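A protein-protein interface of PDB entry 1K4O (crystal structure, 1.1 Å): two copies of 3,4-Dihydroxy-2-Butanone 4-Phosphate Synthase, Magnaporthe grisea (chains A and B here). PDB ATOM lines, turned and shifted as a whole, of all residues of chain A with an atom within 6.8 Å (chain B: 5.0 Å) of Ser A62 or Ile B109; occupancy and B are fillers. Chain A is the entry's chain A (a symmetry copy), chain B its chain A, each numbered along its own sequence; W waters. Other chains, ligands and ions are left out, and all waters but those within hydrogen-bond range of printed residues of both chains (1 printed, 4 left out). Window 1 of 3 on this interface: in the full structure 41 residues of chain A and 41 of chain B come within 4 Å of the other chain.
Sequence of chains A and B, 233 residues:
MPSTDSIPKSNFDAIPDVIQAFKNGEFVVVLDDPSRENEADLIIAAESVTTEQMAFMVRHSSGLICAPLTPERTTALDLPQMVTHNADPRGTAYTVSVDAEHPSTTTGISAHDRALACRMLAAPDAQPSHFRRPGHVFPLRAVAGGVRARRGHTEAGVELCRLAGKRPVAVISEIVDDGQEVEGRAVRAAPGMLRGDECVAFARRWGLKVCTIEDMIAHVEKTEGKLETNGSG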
ATOM      1  N   GLU A  37     -15.938  13.114  26.385  1.00  0.00           N
ATOM      2  CA  GLU A  37     -15.686  12.169  25.304  1.00  0.00           C
ATOM      3  C   GLU A  37     -16.981  11.823  24.562  1.00  0.00           C
ATOM      4  O   GLU A  37     -16.933  11.382  23.400  1.00  0.00           O
ATOM      5  CB  GLU A  37     -15.039  10.875  25.836  1.00  0.00           C
ATOM      6  CG  GLU A  37     -13.734  11.129  26.577  1.00  0.00           C
ATOM      7  CD  GLU A  37     -13.097   9.859  27.017  1.00  0.00           C
ATOM      8  OE1 GLU A  37     -11.990   9.586  26.609  1.00  0.00           O
ATOM      9  OE2 GLU A  37     -13.766   9.078  27.853  1.00  0.00           O
ATOM     10  N   GLU A  39     -18.724   9.315  25.210  1.00  0.00           N
ATOM     11  CA  GLU A  39     -18.575   7.884  25.011  1.00  0.00           C
ATOM     12  C   GLU A  39     -19.176   7.067  26.136  1.00  0.00           C
ATOM     13  O   GLU A  39     -19.215   7.535  27.293  1.00  0.00           O
ATOM     14  CB  GLU A  39     -17.082   7.456  24.880  1.00  0.00           C
ATOM     15  CG  GLU A  39     -16.428   7.922  23.561  1.00  0.00           C
ATOM     16  CD  GLU A  39     -14.934   7.721  23.482  1.00  0.00           C
ATOM     17  OE1 GLU A  39     -14.235   7.319  24.401  1.00  0.00           O
ATOM     18  OE2 GLU A  39     -14.448   8.082  22.310  1.00  0.00           O
ATOM     19  N   MET A  57     -16.623  -8.531  26.400  1.00  0.00           N
ATOM     20  CA  MET A  57     -16.086  -7.177  26.445  1.00  0.00           C
ATOM     21  C   MET A  57     -15.201  -6.881  25.229  1.00  0.00           C
ATOM     22  O   MET A  57     -15.323  -5.817  24.587  1.00  0.00           O
ATOM     23  CB  MET A  57     -15.294  -7.004  27.750  1.00  0.00           C
ATOM     24  CG  MET A  57     -15.032  -5.534  28.075  1.00  0.00           C
ATOM     25  SD  MET A  57     -14.145  -5.408  29.653  1.00  0.00           S
ATOM     26  CE  MET A  57     -14.718  -3.769  30.125  1.00  0.00           C
ATOM     27  N   VAL A  58     -14.343  -7.813  24.899  1.00  0.00           N
ATOM     28  CA  VAL A  58     -13.447  -7.621  23.759  1.00  0.00           C
ATOM     29  C   VAL A  58     -14.235  -7.506  22.480  1.00  0.00           C
ATOM     30  O   VAL A  58     -13.972  -6.679  21.612  1.00  0.00           O
ATOM     31  CB  VAL A  58     -12.437  -8.764  23.707  1.00  0.00           C
ATOM     32  CG1 VAL A  58     -11.600  -8.721  22.409  1.00  0.00           C
ATOM     33  CG2 VAL A  58     -11.460  -8.622  24.887  1.00  0.00           C
ATOM     34  N   ARG A  59     -15.228  -8.375  22.326  1.00  0.00           N
ATOM     35  CA  ARG A  59     -16.033  -8.373  21.117  1.00  0.00           C
ATOM     36  C   ARG A  59     -16.765  -7.072  20.889  1.00  0.00           C
ATOM     37  O   ARG A  59     -16.887  -6.663  19.734  1.00  0.00           O
ATOM     38  CB  ARG A  59     -17.038  -9.523  21.203  1.00  0.00           C
ATOM     39  CG  ARG A  59     -18.188  -9.476  20.168  1.00  0.00           C
ATOM     40  CD  ARG A  59     -17.661  -9.690  18.742  1.00  0.00           C
ATOM     41  NE  ARG A  59     -18.790  -9.618  17.819  1.00  0.00           N
ATOM     42  CZ  ARG A  59     -19.398  -8.476  17.488  1.00  0.00           C
ATOM     43  NH1 ARG A  59     -18.989  -7.254  17.886  1.00  0.00           N
ATOM     44  NH2 ARG A  59     -20.457  -8.594  16.679  1.00  0.00           N
ATOM     45  N   HIS A  60     -17.329  -6.455  21.932  1.00  0.00           N
ATOM     46  CA  HIS A  60     -18.131  -5.269  21.755  1.00  0.00           C
ATOM     47  C   HIS A  60     -17.451  -3.950  22.014  1.00  0.00           C
ATOM     48  O   HIS A  60     -18.037  -2.894  21.777  1.00  0.00           O
ATOM     49  CB  HIS A  60     -19.423  -5.390  22.596  1.00  0.00           C
ATOM     50  CG  HIS A  60     -20.271  -6.529  22.145  1.00  0.00           C
ATOM     51  ND1 HIS A  60     -21.049  -6.435  20.999  1.00  0.00           N
ATOM     52  CD2 HIS A  60     -20.394  -7.802  22.663  1.00  0.00           C
ATOM     53  CE1 HIS A  60     -21.635  -7.623  20.852  1.00  0.00           C
ATOM     54  NE2 HIS A  60     -21.255  -8.483  21.814  1.00  0.00           N
ATOM     55  N   SER A  61     -16.215  -3.969  22.475  1.00  0.00           N
ATOM     56  CA  SER A  61     -15.533  -2.733  22.774  1.00  0.00           C
ATOM     57  C   SER A  61     -14.414  -2.464  21.776  1.00  0.00           C
ATOM     58  O   SER A  61     -14.158  -3.221  20.838  1.00  0.00           O
ATOM     59  CB  SER A  61     -14.952  -2.828  24.203  1.00  0.00           C
ATOM     60  OG  SER A  61     -13.814  -3.681  24.253  1.00  0.00           O
ATOM     61  N   SER A  62     -13.639  -1.417  22.079  1.00  0.00           N
ATOM     62  CA  SER A  62     -12.438  -1.104  21.285  1.00  0.00           C
ATOM     63  C   SER A  62     -11.388  -2.210  21.429  1.00  0.00           C
ATOM     64  O   SER A  62     -10.443  -2.306  20.612  1.00  0.00           O
ATOM     65  CB  SER A  62     -11.858   0.205  21.807  1.00  0.00           C
ATOM     66  OG  SER A  62     -11.298  -0.023  23.097  1.00  0.00           O
ATOM     67  N   GLY A  63     -11.466  -3.028  22.496  1.00  0.00           N
ATOM     68  CA  GLY A  63     -10.420  -4.034  22.691  1.00  0.00           C
ATOM     69  C   GLY A  63      -9.260  -3.520  23.540  1.00  0.00           C
ATOM     70  O   GLY A  63      -8.398  -4.306  23.919  1.00  0.00           O
ATOM     71  N   LEU A  64      -9.239  -2.212  23.832  1.00  0.00           N
ATOM     72  CA  LEU A  64      -8.211  -1.690  24.710  1.00  0.00           C
ATOM     73  C   LEU A  64      -8.819  -1.822  26.106  1.00  0.00           C
ATOM     74  O   LEU A  64      -9.604  -0.968  26.531  1.00  0.00           O
ATOM     75  CB  LEU A  64      -7.810  -0.236  24.392  1.00  0.00           C
ATOM     76  CG  LEU A  64      -6.967  -0.035  23.145  1.00  0.00           C
ATOM     77  CD1 LEU A  64      -6.203   1.299  23.217  1.00  0.00           C
ATOM     78  CD2 LEU A  64      -5.955  -1.164  23.106  1.00  0.00           C
ATOM     79  N   ILE A  65      -8.524  -2.948  26.761  1.00  0.00           N
ATOM     80  CA  ILE A  65      -9.116  -3.294  28.069  1.00  0.00           C
ATOM     81  C   ILE A  65      -8.245  -2.691  29.160  1.00  0.00           C
ATOM     82  O   ILE A  65      -7.073  -3.044  29.275  1.00  0.00           O
ATOM     83  CB  ILE A  65      -9.219  -4.819  28.230  1.00  0.00           C
ATOM     84  CG1 ILE A  65      -9.951  -5.451  27.047  1.00  0.00           C
ATOM     85  CG2 ILE A  65      -9.865  -5.176  29.566  1.00  0.00           C
ATOM     86  CD1 ILE A  65     -11.340  -4.836  26.845  1.00  0.00           C
ATOM     87  N   TYR A  94      -2.585   6.288  32.320  1.00  0.00           N
ATOM     88  CA  TYR A  94      -2.112   4.955  32.101  1.00  0.00           C
ATOM     89  C   TYR A  94      -0.873   4.612  32.926  1.00  0.00           C
ATOM     90  O   TYR A  94       0.090   5.405  32.924  1.00  0.00           O
ATOM     91  CB  TYR A  94      -1.611   4.781  30.638  1.00  0.00           C
ATOM     92  CG  TYR A  94      -2.701   4.977  29.619  1.00  0.00           C
ATOM     93  CD1 TYR A  94      -2.852   6.198  28.964  1.00  0.00           C
ATOM     94  CD2 TYR A  94      -3.555   3.913  29.347  1.00  0.00           C
ATOM     95  CE1 TYR A  94      -3.880   6.372  28.036  1.00  0.00           C
ATOM     96  CE2 TYR A  94      -4.585   4.081  28.423  1.00  0.00           C
ATOM     97  CZ  TYR A  94      -4.739   5.305  27.788  1.00  0.00           C
ATOM     98  OH  TYR A  94      -5.800   5.392  26.908  1.00  0.00           O
ATOM     99  N   ILE A 172     -12.583  -1.406  32.316  1.00  0.00           N
ATOM    100  CA  ILE A 172     -13.352  -0.564  31.444  1.00  0.00           C
ATOM    101  C   ILE A 172     -12.822  -0.643  30.015  1.00  0.00           C
ATOM    102  O   ILE A 172     -11.644  -0.915  29.763  1.00  0.00           O
ATOM    103  CB  ILE A 172     -13.370   0.921  31.865  1.00  0.00           C
ATOM    104  CG1 ILE A 172     -12.011   1.621  31.700  1.00  0.00           C
ATOM    105  CG2 ILE A 172     -13.881   1.085  33.308  1.00  0.00           C
ATOM    106  CD1 ILE A 172     -12.091   3.121  32.041  1.00  0.00           C
ATOM    107  N   SER A 173     -13.721  -0.383  29.065  1.00  0.00           N
ATOM    108  CA  SER A 173     -13.367  -0.275  27.646  1.00  0.00           C
ATOM    109  C   SER A 173     -14.502   0.461  26.931  1.00  0.00           C
ATOM    110  O   SER A 173     -15.693   0.330  27.311  1.00  0.00           O
ATOM    111  CB  SER A 173     -13.016  -1.617  27.011  1.00  0.00           C
ATOM    112  OG  SER A 173     -12.373  -1.361  25.759  1.00  0.00           O
ATOM    113  N   GLU A 174     -14.162   1.228  25.880  1.00  0.00           N
ATOM    114  CA  GLU A 174     -15.157   1.978  25.149  1.00  0.00           C
ATOM    115  C   GLU A 174     -16.005   1.096  24.224  1.00  0.00           C
ATOM    116  O   GLU A 174     -15.486   0.209  23.550  1.00  0.00           O
ATOM    117  CB  GLU A 174     -14.479   3.027  24.243  1.00  0.00           C
ATOM    118  CG  GLU A 174     -13.457   3.904  24.984  1.00  0.00           C
ATOM    119  CD  GLU A 174     -12.060   3.351  24.861  1.00  0.00           C
ATOM    120  OE1 GLU A 174     -11.842   2.141  24.789  1.00  0.00           O
ATOM    121  OE2 GLU A 174     -11.125   4.292  24.802  1.00  0.00           O
ATOM    122  N   ILE A 175     -17.305   1.385  24.157  1.00  0.00           N
ATOM    123  CA  ILE A 175     -18.225   0.666  23.280  1.00  0.00           C
ATOM    124  C   ILE A 175     -18.160   1.322  21.910  1.00  0.00           C
ATOM    125  O   ILE A 175     -18.586   2.449  21.722  1.00  0.00           O
ATOM    126  CB  ILE A 175     -19.662   0.615  23.846  1.00  0.00           C
ATOM    127  CG1 ILE A 175     -19.660  -0.029  25.249  1.00  0.00           C
ATOM    128  CG2 ILE A 175     -20.502  -0.268  22.921  1.00  0.00           C
ATOM    129  CD1 ILE A 175     -21.004   0.129  25.961  1.00  0.00           C
ATOM    130  N   VAL A 176     -17.609   0.602  20.927  1.00  0.00           N
ATOM    131  CA  VAL A 176     -17.496   1.164  19.580  1.00  0.00           C
ATOM    132  C   VAL A 176     -18.719   0.816  18.735  1.00  0.00           C
ATOM    133  O   VAL A 176     -19.563   0.004  19.082  1.00  0.00           O
ATOM    134  CB  VAL A 176     -16.244   0.603  18.871  1.00  0.00           C
ATOM    135  CG1 VAL A 176     -14.979   0.884  19.689  1.00  0.00           C
ATOM    136  CG2 VAL A 176     -16.407  -0.898  18.616  1.00  0.00           C
ATOM    137  N   MET A 193     -18.278   5.441  17.077  1.00  0.00           N
ATOM    138  CA  MET A 193     -18.418   5.187  18.514  1.00  0.00           C
ATOM    139  C   MET A 193     -19.889   5.102  18.818  1.00  0.00           C
ATOM    140  O   MET A 193     -20.641   5.798  18.179  1.00  0.00           O
ATOM    141  CB  MET A 193     -17.760   6.258  19.433  1.00  0.00           C
ATOM    142  CG  MET A 193     -16.264   6.370  19.174  1.00  0.00           C
ATOM    143  SD  MET A 193     -15.367   4.817  19.370  1.00  0.00           S
ATOM    144  CE  MET A 193     -15.481   4.681  21.183  1.00  0.00           C
ATOM    145  N   VAL B  58     -10.336  -4.014  14.111  1.00  0.00           N
ATOM    146  CA  VAL B  58     -10.770  -3.967  15.507  1.00  0.00           C
ATOM    147  C   VAL B  58     -11.806  -5.027  15.775  1.00  0.00           C
ATOM    148  O   VAL B  58     -11.801  -5.716  16.791  1.00  0.00           O
ATOM    149  CB  VAL B  58     -11.286  -2.568  15.833  1.00  0.00           C
ATOM    150  CG1 VAL B  58     -11.944  -2.519  17.230  1.00  0.00           C
ATOM    151  CG2 VAL B  58     -10.099  -1.589  15.851  1.00  0.00           C
ATOM    152  N   SER B  62      -7.922  -8.796  18.658  1.00  0.00           N
ATOM    153  CA  SER B  62      -7.951  -8.501  20.101  1.00  0.00           C
ATOM    154  C   SER B  62      -8.293  -7.029  20.349  1.00  0.00           C
ATOM    155  O   SER B  62      -8.676  -6.641  21.478  1.00  0.00           O
ATOM    156  CB  SER B  62      -6.566  -8.792  20.666  1.00  0.00           C
ATOM    157  OG  SER B  62      -5.658  -7.804  20.190  1.00  0.00           O
ATOM    158  N   GLY B  63      -8.102  -6.152  19.344  1.00  0.00           N
ATOM    159  CA  GLY B  63      -8.345  -4.730  19.594  1.00  0.00           C
ATOM    160  C   GLY B  63      -7.097  -3.996  20.079  1.00  0.00           C
ATOM    161  O   GLY B  63      -7.114  -2.773  20.167  1.00  0.00           O
ATOM    162  N   THR B 107     -11.028  11.304  20.664  1.00  0.00           N
ATOM    163  CA  THR B 107     -10.481  10.611  21.833  1.00  0.00           C
ATOM    164  C   THR B 107      -9.315   9.677  21.549  1.00  0.00           C
ATOM    165  O   THR B 107      -8.688   9.164  22.492  1.00  0.00           O
ATOM    166  CB  THR B 107     -11.593   9.830  22.565  1.00  0.00           C
ATOM    167  OG1 THR B 107     -12.090   8.882  21.644  1.00  0.00           O
ATOM    168  CG2 THR B 107     -12.771  10.714  22.940  1.00  0.00           C
ATOM    169  N   GLY B 108      -9.016   9.450  20.272  1.00  0.00           N
ATOM    170  CA  GLY B 108      -7.928   8.565  19.941  1.00  0.00           C
ATOM    171  C   GLY B 108      -8.278   7.098  19.755  1.00  0.00           C
ATOM    172  O   GLY B 108      -7.462   6.349  19.214  1.00  0.00           O
ATOM    173  N   ILE B 109      -9.464   6.669  20.196  1.00  0.00           N
ATOM    174  CA  ILE B 109      -9.787   5.248  20.114  1.00  0.00           C
ATOM    175  C   ILE B 109     -10.595   4.799  18.892  1.00  0.00           C
ATOM    176  O   ILE B 109     -10.581   3.614  18.554  1.00  0.00           O
ATOM    177  CB  ILE B 109     -10.515   4.824  21.413  1.00  0.00           C
ATOM    178  CG1 ILE B 109     -10.586   3.311  21.566  1.00  0.00           C
ATOM    179  CG2 ILE B 109     -11.942   5.384  21.419  1.00  0.00           C
ATOM    180  CD1 ILE B 109      -9.228   2.662  21.772  1.00  0.00           C
ATOM    181  N   SER B 110     -11.311   5.700  18.257  1.00  0.00           N
ATOM    182  CA  SER B 110     -12.143   5.242  17.157  1.00  0.00           C
ATOM    183  C   SER B 110     -11.341   4.628  16.027  1.00  0.00           C
ATOM    184  O   SER B 110     -10.144   4.915  15.871  1.00  0.00           O
ATOM    185  CB  SER B 110     -12.972   6.389  16.608  1.00  0.00           C
ATOM    186  OG  SER B 110     -12.093   7.317  15.977  1.00  0.00           O
ATOM    187  N   ALA B 111     -12.009   3.857  15.186  1.00  0.00           N
ATOM    188  CA  ALA B 111     -11.332   3.329  13.983  1.00  0.00           C
ATOM    189  C   ALA B 111     -10.718   4.471  13.190  1.00  0.00           C
ATOM    190  O   ALA B 111      -9.602   4.349  12.661  1.00  0.00           O
ATOM    191  CB  ALA B 111     -12.276   2.526  13.082  1.00  0.00           C
ATOM    192  N   ASP B 113      -9.623   7.402  14.277  1.00  0.00           N
ATOM    193  CA  ASP B 113      -8.444   7.942  14.961  1.00  0.00           C
ATOM    194  C   ASP B 113      -7.256   6.998  14.970  1.00  0.00           C
ATOM    195  O   ASP B 113      -6.124   7.428  14.799  1.00  0.00           O
ATOM    196  CB  ASP B 113      -8.787   8.403  16.400  1.00  0.00           C
ATOM    197  CG  ASP B 113      -9.704   9.601  16.433  1.00  0.00           C
ATOM    198  OD1 ASP B 113     -10.112  10.140  15.411  1.00  0.00           O
ATOM    199  OD2 ASP B 113      -9.968  10.040  17.625  1.00  0.00           O
ATOM    200  N   ARG B 114      -7.498   5.710  15.193  1.00  0.00           N
ATOM    201  CA  ARG B 114      -6.379   4.771  15.220  1.00  0.00           C
ATOM    202  C   ARG B 114      -5.770   4.630  13.827  1.00  0.00           C
ATOM    203  O   ARG B 114      -4.546   4.541  13.683  1.00  0.00           O
ATOM    204  CB  ARG B 114      -6.750   3.436  15.874  1.00  0.00           C
ATOM    205  CG  ARG B 114      -6.966   3.629  17.379  1.00  0.00           C
ATOM    206  CD  ARG B 114      -6.965   2.291  18.142  1.00  0.00           C
ATOM    207  NE  ARG B 114      -8.306   1.692  18.203  1.00  0.00           N
ATOM    208  CZ  ARG B 114      -8.519   0.531  18.862  1.00  0.00           C
ATOM    209  NH1 ARG B 114      -7.513  -0.175  19.417  1.00  0.00           N
ATOM    210  NH2 ARG B 114      -9.738   0.024  18.916  1.00  0.00           N
ATOM    211  N   HIS B 136      -3.494   5.583  22.142  1.00  0.00           N
ATOM    212  CA  HIS B 136      -4.221   4.355  21.883  1.00  0.00           C
ATOM    213  C   HIS B 136      -3.721   3.424  20.821  1.00  0.00           C
ATOM    214  O   HIS B 136      -4.375   2.429  20.541  1.00  0.00           O
ATOM    215  CB  HIS B 136      -5.729   4.669  21.689  1.00  0.00           C
ATOM    216  CG  HIS B 136      -6.315   5.533  22.770  1.00  0.00           C
ATOM    217  ND1 HIS B 136      -6.094   6.905  22.818  1.00  0.00           N
ATOM    218  CD2 HIS B 136      -7.099   5.217  23.831  1.00  0.00           C
ATOM    219  CE1 HIS B 136      -6.711   7.390  23.894  1.00  0.00           C
ATOM    220  NE2 HIS B 136      -7.341   6.387  24.517  1.00  0.00           N
HETATM  221  O   HOH W   1     -11.663  -5.563  19.880  1.00  0.00           O
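Among the printed residues, pairs that only touch across the chains: Glu A37 with Thr B107 (3.7 Å), Glu A39 with Ile B109 (3.8 Å), Val A58 with Ser B62 (3.7 Å), Ser A62 with Val B58 (3.7 Å), Ser A62 with Ile B109 (3.4 Å), Gly A63 with Gly B63 (3.8 Å), Leu A64 with Gly B63 (3.5 Å), Leu A64 with Ile B109 (3.6 Å), Leu A64 with Arg B114 (3.8 Å), Leu A64 with His B136 (3.4 Å), Glu A174 with Ile B109 (3.4 Å), Met A193 with Ile B109 (3.6 Å) and Met A193 with Ser B110 (3.9 Å).
Of the 18 printed residues of chain A, 9 touch a printed residue of chain B.
The guanidinium group (NH1) of Arg B114 lies within hydrogen-bond range of the backbone carbonyl oxygen (O) of Gly B63 (2.7 Å). N of Thr B107 is in hydrogen-bond range of OD2 of Asp B113 (3.5 Å). A ring nitrogen (ND1) of His B136 lies close to the backbone carbonyl oxygen of Thr B107. The backbone NH (N) of Leu A64 is in hydrogen-bond range of the side-chain hydroxyl (OG) of Ser A62, at 3.1 Å. The side-chain hydroxyl (OG) of Ser A62 sits at hydrogen-bond distance from the side-chain hydroxyl (OG) of Ser A173 (3.2 Å). The side-chain hydroxyl (OG) of Ser A173 lies within hydrogen-bond range of the backbone carbonyl oxygen (O) of Leu A64 (2.9 Å).
The side-chain hydroxyl of Thr B107 lies within hydrogen-bond range of the side-chain carboxylate of Glu A39. The guanidinium group of Arg B114 lies within hydrogen-bond range of the backbone carbonyl oxygen of Ser A62, 3.0 Å away. OH of Tyr A94 sits at hydrogen-bond distance from NE2 of His B136, 3.0 Å away. The backbone carbonyl oxygen of Gly B63 lies close to the backbone carbonyl oxygen of Ser A62. O of Gly A63 sits close to O of Ser B62 (3.4 Å).
Printed residues of chain B within 4 Å of Glu A37: Thr B107 (3.7 Å). Of the printed residues of chain B, Ser A62 touches Val B58, Gly B63, Ile B109 and Arg B114. Ile A65 touches none of the printed residues of chain B. Of the printed residues of chain A, Val B58 touches Ser A62. Of the printed residues of chain A, His B136 touches Leu A64 (3.4 Å) and Tyr A94 (3.0 Å). The nearest printed residue of chain A that does not touch His B136 is Glu A174 (4.2 Å).
Val A58 touches Ser B62, and with the chains exchanged Ser A62 touches Val B58. Ser A62 touches Gly B63, and with the chains exchanged Gly A63 touches Ser B62. Gly A63 touches its own counterpart, Gly B63. 3 positions are printed for both chains. Of the 18 pairs that touch across the chains among the printed residues, 5 have their exchanged pair printed and touching as well.
Water W1 lies within hydrogen-bond range of the backbone carbonyl oxygen (O) of Val B58 (3.1 Å) and the backbone carbonyl oxygen (O) of Val A58 (3.1 Å).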
